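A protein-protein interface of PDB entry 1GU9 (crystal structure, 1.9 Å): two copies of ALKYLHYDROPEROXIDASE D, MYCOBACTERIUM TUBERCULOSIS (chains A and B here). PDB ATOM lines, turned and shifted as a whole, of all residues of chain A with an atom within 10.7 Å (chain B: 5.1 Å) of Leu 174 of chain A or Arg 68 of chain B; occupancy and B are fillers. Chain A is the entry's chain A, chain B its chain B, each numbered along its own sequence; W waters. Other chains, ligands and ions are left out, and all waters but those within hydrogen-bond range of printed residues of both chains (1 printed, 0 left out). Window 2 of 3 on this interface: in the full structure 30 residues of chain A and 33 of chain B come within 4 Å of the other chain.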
ATOM      1  N   ALA A   9      31.658  -1.748 -10.934  1.00  0.00           N
ATOM      2  CA  ALA A   9      31.553  -2.796  -9.921  1.00  0.00           C
ATOM      3  C   ALA A   9      30.656  -2.418  -8.743  1.00  0.00           C
ATOM      4  O   ALA A   9      30.347  -3.269  -7.913  1.00  0.00           O
ATOM      5  CB  ALA A   9      32.943  -3.168  -9.409  1.00  0.00           C
ATOM      6  N   PRO A  11      27.361  -1.715  -6.649  1.00  0.00           N
ATOM      7  CA  PRO A  11      25.974  -2.190  -6.590  1.00  0.00           C
ATOM      8  C   PRO A  11      24.944  -1.102  -6.820  1.00  0.00           C
ATOM      9  O   PRO A  11      25.286   0.078  -6.898  1.00  0.00           O
ATOM     10  CB  PRO A  11      25.873  -2.785  -5.190  1.00  0.00           C
ATOM     11  CG  PRO A  11      26.835  -1.951  -4.404  1.00  0.00           C
ATOM     12  CD  PRO A  11      28.014  -1.862  -5.335  1.00  0.00           C
ATOM     13  N   GLU A  12      23.681  -1.509  -6.928  1.00  0.00           N
ATOM     14  CA  GLU A  12      22.588  -0.568  -7.154  1.00  0.00           C
ATOM     15  C   GLU A  12      22.198   0.181  -5.888  1.00  0.00           C
ATOM     16  O   GLU A  12      21.707   1.316  -5.951  1.00  0.00           O
ATOM     17  CB  GLU A  12      21.368  -1.292  -7.727  1.00  0.00           C
ATOM     18  CG  GLU A  12      21.457  -1.562  -9.222  1.00  0.00           C
ATOM     19  CD  GLU A  12      21.693  -0.292 -10.028  1.00  0.00           C
ATOM     20  OE1 GLU A  12      20.957   0.701  -9.815  1.00  0.00           O
ATOM     21  OE2 GLU A  12      22.612  -0.288 -10.878  1.00  0.00           O
ATOM     22  N   TYR A  13      22.422  -0.448  -4.739  1.00  0.00           N
ATOM     23  CA  TYR A  13      22.110   0.192  -3.467  1.00  0.00           C
ATOM     24  C   TYR A  13      23.241   1.119  -3.062  1.00  0.00           C
ATOM     25  O   TYR A  13      23.316   1.561  -1.923  1.00  0.00           O
ATOM     26  CB  TYR A  13      21.868  -0.854  -2.377  1.00  0.00           C
ATOM     27  CG  TYR A  13      22.927  -1.922  -2.254  1.00  0.00           C
ATOM     28  CD1 TYR A  13      24.178  -1.631  -1.726  1.00  0.00           C
ATOM     29  CD2 TYR A  13      22.665  -3.235  -2.645  1.00  0.00           C
ATOM     30  CE1 TYR A  13      25.134  -2.609  -1.585  1.00  0.00           C
ATOM     31  CE2 TYR A  13      23.622  -4.225  -2.510  1.00  0.00           C
ATOM     32  CZ  TYR A  13      24.859  -3.899  -1.976  1.00  0.00           C
ATOM     33  OH  TYR A  13      25.826  -4.857  -1.837  1.00  0.00           O
ATOM     34  N   ALA A  14      24.121   1.406  -4.016  1.00  0.00           N
ATOM     35  CA  ALA A  14      25.259   2.283  -3.786  1.00  0.00           C
ATOM     36  C   ALA A  14      25.382   3.248  -4.950  1.00  0.00           C
ATOM     37  O   ALA A  14      26.481   3.537  -5.422  1.00  0.00           O
ATOM     38  CB  ALA A  14      26.540   1.455  -3.643  1.00  0.00           C
ATOM     39  N   GLN A 166      33.737   0.742   0.978  1.00  0.00           N
ATOM     40  CA  GLN A 166      32.702   0.038   1.740  1.00  0.00           C
ATOM     41  C   GLN A 166      31.759  -0.672   0.757  1.00  0.00           C
ATOM     42  O   GLN A 166      31.486  -1.869   0.893  1.00  0.00           O
ATOM     43  CB  GLN A 166      31.891   1.019   2.564  1.00  0.00           C
ATOM     44  CG  GLN A 166      30.679   0.375   3.251  1.00  0.00           C
ATOM     45  CD  GLN A 166      31.080  -0.623   4.328  1.00  0.00           C
ATOM     46  OE1 GLN A 166      31.327  -1.799   4.056  1.00  0.00           O
ATOM     47  NE2 GLN A 166      31.171  -0.146   5.552  1.00  0.00           N
ATOM     48  N   ALA A 167      31.279   0.077  -0.229  1.00  0.00           N
ATOM     49  CA  ALA A 167      30.360  -0.466  -1.238  1.00  0.00           C
ATOM     50  C   ALA A 167      30.984  -1.673  -1.945  1.00  0.00           C
ATOM     51  O   ALA A 167      30.340  -2.702  -2.098  1.00  0.00           O
ATOM     52  CB  ALA A 167      30.009   0.613  -2.246  1.00  0.00           C
ATOM     53  N   LEU A 168      32.254  -1.549  -2.327  1.00  0.00           N
ATOM     54  CA  LEU A 168      32.982  -2.621  -3.027  1.00  0.00           C
ATOM     55  C   LEU A 168      33.252  -3.853  -2.157  1.00  0.00           C
ATOM     56  O   LEU A 168      33.167  -5.001  -2.618  1.00  0.00           O
ATOM     57  CB  LEU A 168      34.307  -2.062  -3.551  1.00  0.00           C
ATOM     58  CG  LEU A 168      34.669  -2.294  -5.019  1.00  0.00           C
ATOM     59  CD1 LEU A 168      33.710  -1.520  -5.911  1.00  0.00           C
ATOM     60  CD2 LEU A 168      36.101  -1.848  -5.262  1.00  0.00           C
ATOM     61  N   ALA A 169      33.598  -3.615  -0.897  1.00  0.00           N
ATOM     62  CA  ALA A 169      33.867  -4.706   0.026  1.00  0.00           C
ATOM     63  C   ALA A 169      32.604  -5.557   0.192  1.00  0.00           C
ATOM     64  O   ALA A 169      32.674  -6.784   0.255  1.00  0.00           O
ATOM     65  CB  ALA A 169      34.320  -4.149   1.394  1.00  0.00           C
ATOM     66  N   THR A 170      31.444  -4.911   0.231  1.00  0.00           N
ATOM     67  CA  THR A 170      30.213  -5.667   0.431  1.00  0.00           C
ATOM     68  C   THR A 170      29.838  -6.530  -0.767  1.00  0.00           C
ATOM     69  O   THR A 170      29.447  -7.680  -0.603  1.00  0.00           O
ATOM     70  CB  THR A 170      29.032  -4.746   0.781  1.00  0.00           C
ATOM     71  OG1 THR A 170      28.723  -3.894  -0.333  1.00  0.00           O
ATOM     72  CG2 THR A 170      29.382  -3.895   1.987  1.00  0.00           C
ATOM     73  N   ILE A 171      29.961  -5.984  -1.969  1.00  0.00           N
ATOM     74  CA  ILE A 171      29.621  -6.757  -3.152  1.00  0.00           C
ATOM     75  C   ILE A 171      30.518  -7.972  -3.305  1.00  0.00           C
ATOM     76  O   ILE A 171      30.040  -9.062  -3.612  1.00  0.00           O
ATOM     77  CB  ILE A 171      29.720  -5.913  -4.423  1.00  0.00           C
ATOM     78  CG1 ILE A 171      28.640  -4.846  -4.396  1.00  0.00           C
ATOM     79  CG2 ILE A 171      29.527  -6.795  -5.659  1.00  0.00           C
ATOM     80  CD1 ILE A 171      27.246  -5.429  -4.361  1.00  0.00           C
ATOM     81  N   GLU A 172      31.818  -7.795  -3.096  1.00  0.00           N
ATOM     82  CA  GLU A 172      32.729  -8.928  -3.241  1.00  0.00           C
ATOM     83  C   GLU A 172      32.467 -10.043  -2.251  1.00  0.00           C
ATOM     84  O   GLU A 172      32.517 -11.206  -2.635  1.00  0.00           O
ATOM     85  CB  GLU A 172      34.175  -8.481  -3.118  1.00  0.00           C
ATOM     86  CG  GLU A 172      34.846  -8.242  -4.469  1.00  0.00           C
ATOM     87  CD  GLU A 172      35.689  -6.977  -4.453  1.00  0.00           C
ATOM     88  OE1 GLU A 172      35.092  -5.896  -4.210  1.00  0.00           O
ATOM     89  OE2 GLU A 172      36.930  -7.055  -4.668  1.00  0.00           O
ATOM     90  N   ALA A 173      32.196  -9.698  -0.985  1.00  0.00           N
ATOM     91  CA  ALA A 173      31.927 -10.709   0.039  1.00  0.00           C
ATOM     92  C   ALA A 173      30.575 -11.387  -0.166  1.00  0.00           C
ATOM     93  O   ALA A 173      30.389 -12.539   0.220  1.00  0.00           O
ATOM     94  CB  ALA A 173      31.992 -10.088   1.448  1.00  0.00           C
ATOM     95  N   LEU A 174      29.623 -10.672  -0.753  1.00  0.00           N
ATOM     96  CA  LEU A 174      28.304 -11.251  -0.992  1.00  0.00           C
ATOM     97  C   LEU A 174      28.220 -11.991  -2.334  1.00  0.00           C
ATOM     98  O   LEU A 174      27.558 -13.032  -2.443  1.00  0.00           O
ATOM     99  CB  LEU A 174      27.229 -10.163  -0.902  1.00  0.00           C
ATOM    100  CG  LEU A 174      26.946  -9.696   0.528  1.00  0.00           C
ATOM    101  CD1 LEU A 174      25.913  -8.600   0.509  1.00  0.00           C
ATOM    102  CD2 LEU A 174      26.459 -10.874   1.365  1.00  0.00           C
ATOM    103  N   SER A 175      28.896 -11.460  -3.348  1.00  0.00           N
ATOM    104  CA  SER A 175      28.909 -12.081  -4.668  1.00  0.00           C
ATOM    105  C   SER A 175      30.224 -12.837  -4.818  1.00  0.00           C
ATOM    106  O   SER A 175      30.329 -13.969  -4.291  1.00  0.00           O
ATOM    107  CB  SER A 175      28.814 -11.011  -5.763  1.00  0.00           C
ATOM    108  OG  SER A 175      27.659 -10.201  -5.604  1.00  0.00           O
ATOM    109  N   LEU B  40      22.987  -7.110   9.447  1.00  0.00           N
ATOM    110  CA  LEU B  40      23.504  -7.074   8.089  1.00  0.00           C
ATOM    111  C   LEU B  40      24.267  -5.781   7.773  1.00  0.00           C
ATOM    112  O   LEU B  40      25.383  -5.837   7.239  1.00  0.00           O
ATOM    113  CB  LEU B  40      22.361  -7.291   7.091  1.00  0.00           C
ATOM    114  CG  LEU B  40      22.755  -7.281   5.617  1.00  0.00           C
ATOM    115  CD1 LEU B  40      23.766  -8.387   5.339  1.00  0.00           C
ATOM    116  CD2 LEU B  40      21.512  -7.456   4.763  1.00  0.00           C
ATOM    117  N   LEU B  52      30.040 -11.060   6.787  1.00  0.00           N
ATOM    118  CA  LEU B  52      29.013 -10.517   5.911  1.00  0.00           C
ATOM    119  C   LEU B  52      28.360 -11.646   5.111  1.00  0.00           C
ATOM    120  O   LEU B  52      27.149 -11.659   4.916  1.00  0.00           O
ATOM    121  CB  LEU B  52      29.625  -9.501   4.949  1.00  0.00           C
ATOM    122  CG  LEU B  52      28.632  -8.821   4.004  1.00  0.00           C
ATOM    123  CD1 LEU B  52      27.465  -8.244   4.799  1.00  0.00           C
ATOM    124  CD2 LEU B  52      29.343  -7.733   3.208  1.00  0.00           C
ATOM    125  N   ALA B  53      29.180 -12.585   4.653  1.00  0.00           N
ATOM    126  CA  ALA B  53      28.704 -13.709   3.856  1.00  0.00           C
ATOM    127  C   ALA B  53      27.756 -14.595   4.663  1.00  0.00           C
ATOM    128  O   ALA B  53      26.679 -14.946   4.189  1.00  0.00           O
ATOM    129  CB  ALA B  53      29.897 -14.524   3.339  1.00  0.00           C
ATOM    130  N   GLY B  56      24.695 -12.399   5.694  1.00  0.00           N
ATOM    131  CA  GLY B  56      23.970 -12.044   4.487  1.00  0.00           C
ATOM    132  C   GLY B  56      23.112 -13.196   3.994  1.00  0.00           C
ATOM    133  O   GLY B  56      21.998 -13.000   3.507  1.00  0.00           O
ATOM    134  N   ALA B  57      23.635 -14.409   4.125  1.00  0.00           N
ATOM    135  CA  ALA B  57      22.913 -15.593   3.688  1.00  0.00           C
ATOM    136  C   ALA B  57      21.731 -15.876   4.611  1.00  0.00           C
ATOM    137  O   ALA B  57      20.626 -16.175   4.151  1.00  0.00           O
ATOM    138  CB  ALA B  57      23.854 -16.792   3.651  1.00  0.00           C
ATOM    139  N   ALA B  59      20.202 -13.789   6.309  1.00  0.00           N
ATOM    140  CA  ALA B  59      19.312 -12.636   6.329  1.00  0.00           C
ATOM    141  C   ALA B  59      18.252 -12.680   5.232  1.00  0.00           C
ATOM    142  O   ALA B  59      17.267 -11.950   5.291  1.00  0.00           O
ATOM    143  CB  ALA B  59      20.122 -11.363   6.208  1.00  0.00           C
ATOM    144  N   THR B  60      18.459 -13.530   4.231  1.00  0.00           N
ATOM    145  CA  THR B  60      17.514 -13.646   3.125  1.00  0.00           C
ATOM    146  C   THR B  60      16.172 -14.241   3.548  1.00  0.00           C
ATOM    147  O   THR B  60      15.118 -13.794   3.091  1.00  0.00           O
ATOM    148  CB  THR B  60      18.089 -14.512   1.998  1.00  0.00           C
ATOM    149  OG1 THR B  60      18.524 -15.765   2.537  1.00  0.00           O
ATOM    150  CG2 THR B  60      19.253 -13.805   1.322  1.00  0.00           C
ATOM    151  N   LEU B  63      14.753 -11.294   5.835  1.00  0.00           N
ATOM    152  CA  LEU B  63      14.546  -9.935   5.319  1.00  0.00           C
ATOM    153  C   LEU B  63      13.967  -9.932   3.912  1.00  0.00           C
ATOM    154  O   LEU B  63      14.302 -10.779   3.080  1.00  0.00           O
ATOM    155  CB  LEU B  63      15.867  -9.143   5.268  1.00  0.00           C
ATOM    156  CG  LEU B  63      16.633  -8.590   6.478  1.00  0.00           C
ATOM    157  CD1 LEU B  63      17.754  -7.712   5.949  1.00  0.00           C
ATOM    158  CD2 LEU B  63      15.727  -7.762   7.387  1.00  0.00           C
ATOM    159  N   SER B  64      13.112  -8.955   3.640  1.00  0.00           N
ATOM    160  CA  SER B  64      12.515  -8.818   2.322  1.00  0.00           C
ATOM    161  C   SER B  64      13.652  -8.467   1.373  1.00  0.00           C
ATOM    162  O   SER B  64      14.804  -8.397   1.787  1.00  0.00           O
ATOM    163  CB  SER B  64      11.495  -7.685   2.326  1.00  0.00           C
ATOM    164  OG  SER B  64      12.139  -6.450   2.564  1.00  0.00           O
ATOM    165  N   ALA B  65      13.335  -8.244   0.103  1.00  0.00           N
ATOM    166  CA  ALA B  65      14.362  -7.880  -0.864  1.00  0.00           C
ATOM    167  C   ALA B  65      14.708  -6.415  -0.630  1.00  0.00           C
ATOM    168  O   ALA B  65      15.874  -6.049  -0.491  1.00  0.00           O
ATOM    169  CB  ALA B  65      13.848  -8.078  -2.287  1.00  0.00           C
ATOM    170  N   ALA B  66      13.681  -5.576  -0.582  1.00  0.00           N
ATOM    171  CA  ALA B  66      13.880  -4.152  -0.355  1.00  0.00           C
ATOM    172  C   ALA B  66      14.651  -3.891   0.943  1.00  0.00           C
ATOM    173  O   ALA B  66      15.452  -2.963   1.017  1.00  0.00           O
ATOM    174  CB  ALA B  66      12.542  -3.446  -0.307  1.00  0.00           C
ATOM    175  N   ALA B  67      14.411  -4.713   1.961  1.00  0.00           N
ATOM    176  CA  ALA B  67      15.080  -4.540   3.248  1.00  0.00           C
ATOM    177  C   ALA B  67      16.573  -4.773   3.083  1.00  0.00           C
ATOM    178  O   ALA B  67      17.379  -3.910   3.408  1.00  0.00           O
ATOM    179  CB  ALA B  67      14.507  -5.509   4.289  1.00  0.00           C
ATOM    180  N   ARG B  68      16.924  -5.952   2.582  1.00  0.00           N
ATOM    181  CA  ARG B  68      18.317  -6.334   2.354  1.00  0.00           C
ATOM    182  C   ARG B  68      19.056  -5.265   1.561  1.00  0.00           C
ATOM    183  O   ARG B  68      20.258  -5.071   1.730  1.00  0.00           O
ATOM    184  CB  ARG B  68      18.375  -7.650   1.579  1.00  0.00           C
ATOM    185  CG  ARG B  68      19.770  -8.130   1.287  1.00  0.00           C
ATOM    186  CD  ARG B  68      19.767  -9.268   0.295  1.00  0.00           C
ATOM    187  NE  ARG B  68      21.076  -9.906   0.215  1.00  0.00           N
ATOM    188  CZ  ARG B  68      21.544 -10.764   1.116  1.00  0.00           C
ATOM    189  NH1 ARG B  68      20.805 -11.092   2.169  1.00  0.00           N
ATOM    190  NH2 ARG B  68      22.754 -11.292   0.967  1.00  0.00           N
ATOM    191  N   HIS B  69      18.318  -4.573   0.702  1.00  0.00           N
ATOM    192  CA  HIS B  69      18.866  -3.525  -0.150  1.00  0.00           C
ATOM    193  C   HIS B  69      19.121  -2.235   0.613  1.00  0.00           C
ATOM    194  O   HIS B  69      20.174  -1.608   0.463  1.00  0.00           O
ATOM    195  CB  HIS B  69      17.894  -3.276  -1.314  1.00  0.00           C
ATOM    196  CG  HIS B  69      18.398  -2.322  -2.354  1.00  0.00           C
ATOM    197  ND1 HIS B  69      18.325  -0.952  -2.211  1.00  0.00           N
ATOM    198  CD2 HIS B  69      18.960  -2.545  -3.567  1.00  0.00           C
ATOM    199  CE1 HIS B  69      18.817  -0.372  -3.293  1.00  0.00           C
ATOM    200  NE2 HIS B  69      19.210  -1.317  -4.131  1.00  0.00           N
ATOM    201  N   ALA B  70      18.152  -1.840   1.429  1.00  0.00           N
ATOM    202  CA  ALA B  70      18.248  -0.623   2.218  1.00  0.00           C
ATOM    203  C   ALA B  70      19.337  -0.762   3.290  1.00  0.00           C
ATOM    204  O   ALA B  70      20.031   0.200   3.608  1.00  0.00           O
ATOM    205  CB  ALA B  70      16.909  -0.332   2.880  1.00  0.00           C
ATOM    206  N   ALA B  71      19.463  -1.960   3.853  1.00  0.00           N
ATOM    207  CA  ALA B  71      20.469  -2.235   4.880  1.00  0.00           C
ATOM    208  C   ALA B  71      21.894  -2.090   4.329  1.00  0.00           C
ATOM    209  O   ALA B  71      22.721  -1.405   4.919  1.00  0.00           O
ATOM    210  CB  ALA B  71      20.277  -3.648   5.449  1.00  0.00           C
ATOM    211  N   LEU B  72      22.172  -2.738   3.202  1.00  0.00           N
ATOM    212  CA  LEU B  72      23.499  -2.669   2.593  1.00  0.00           C
ATOM    213  C   LEU B  72      23.784  -1.282   2.073  1.00  0.00           C
ATOM    214  O   LEU B  72      24.937  -0.836   2.065  1.00  0.00           O
ATOM    215  CB  LEU B  72      23.620  -3.708   1.477  1.00  0.00           C
ATOM    216  CG  LEU B  72      23.536  -5.158   1.937  1.00  0.00           C
ATOM    217  CD1 LEU B  72      23.550  -6.067   0.716  1.00  0.00           C
ATOM    218  CD2 LEU B  72      24.707  -5.505   2.851  1.00  0.00           C
HETATM  219  O   HOH W   1      27.743  -1.565   1.645  1.00  0.00           O
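The backbone NH of Tyr 13 of chain A lies close to a ring nitrogen (NE2) of His 69 of chain B (3.4 Å).
OH of Tyr 13 of chain A is in hydrogen-bond range of OG1 of Thr 170 of chain A, at 3.4 Å.
O of Ala 167 of chain A is in hydrogen-bond range of OG1 of Thr 170 of chain A.
NH1 of Arg 68 of chain B is in hydrogen-bond range of O of Gly 56 of chain B (2.6 Å).
Among the printed residues, merely in contact across the chains: Glu 12 of chain A with His 69 of chain B (3.8 Å), Tyr 13 of chain A with Leu 72 of chain B (3.6 Å), Thr 170 of chain A with Leu 52 of chain B (3.6 Å), Ala 173 of chain A with Leu 52 of chain B (3.96 Å), Ala 173 of chain A with Ala 53 of chain B (3.7 Å), Leu 174 of chain A with Leu 52 of chain B (3.7 Å), Leu 174 of chain A with Arg 68 of chain B (3.7 Å) and Leu 174 of chain A with Leu 72 of chain B (3.5 Å).
Leu 174 of chain A touches three residues of chain B.
Of chain A, only Leu 174 comes within 4 Å of Arg 68 of chain B.
Of chain A, only Thr 170 (3.6 Å), Ala 173 (3.96 Å) and Leu 174 (3.7 Å) come within 4 Å of Leu 52 of chain B.
No residue of chain A comes within 4 Å of Gly 56 of chain B.
No residue of chain A comes within 4 Å of Ala 59 of chain B.
Thr 60 of chain B touches none of the printed residues of chain A.
No residue of chain A comes within 4 Å of Leu 63 of chain B.
No residue of chain A comes within 4 Å of Ser 64 of chain B.
No residue of chain A comes within 4 Å of Ala 70 of chain B.
No residue of chain A comes within 4 Å of Ala 71 of chain B.
Printed residues of chain A within 4 Å of Leu 72 of chain B: Tyr 13 (3.6 Å) and Leu 174 (3.5 Å).
Printed residues of chain B within 4 Å of Thr 170 of chain A: Leu 52 (3.6 Å).
Printed residues of chain A within 4 Å of His 69 of chain B: Glu 12 (3.8 Å) and Tyr 13 (3.2 Å).
Printed residues of chain B within 4 Å of Tyr 13 of chain A: His 69 (3.2 Å) and Leu 72 (3.6 Å).
Of the printed residues of chain B, Glu 12 of chain A touches His 69.
The nearest residue of chain B that does not touch Leu 174 of chain A is Gly 56 of chain B (4.2 Å).
The nearest residue of chain A that does not touch Arg 68 of chain B is Tyr 13 of chain A (5.3 Å).
The nearest printed residue of chain B that does not touch Thr 170 of chain A is Leu 72 of chain B (4.9 Å).
Hydrophobic or aromatic side chains of chain A within 4 Å of the printed part of chain B: Tyr 13, Ala 173 and Leu 174.
Along chain A the printed residues that touch a printed residue of chain B span positions 12 to 174.
Hydrophobic or aromatic side chains of chain B that line the printed part of chain A: Leu 52, Ala 53, His 69 and Leu 72.
Among the printed residues, 9 pairs touch across the chains.
Among the printed residues, no Asp or Glu carboxylate lies within 4 Å of a Lys or Arg side-chain nitrogen of the other chain.
No position is printed for both chains.
Of the 9 pairs that touch across the chains among the printed residues, none has its exchanged pair printed and touching as well.
Water W1 bridges the backbone carbonyl oxygen of Leu 72 of chain B (2.9 Å) and the side-chain hydroxyl of Thr 170 of chain A (3.2 Å).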
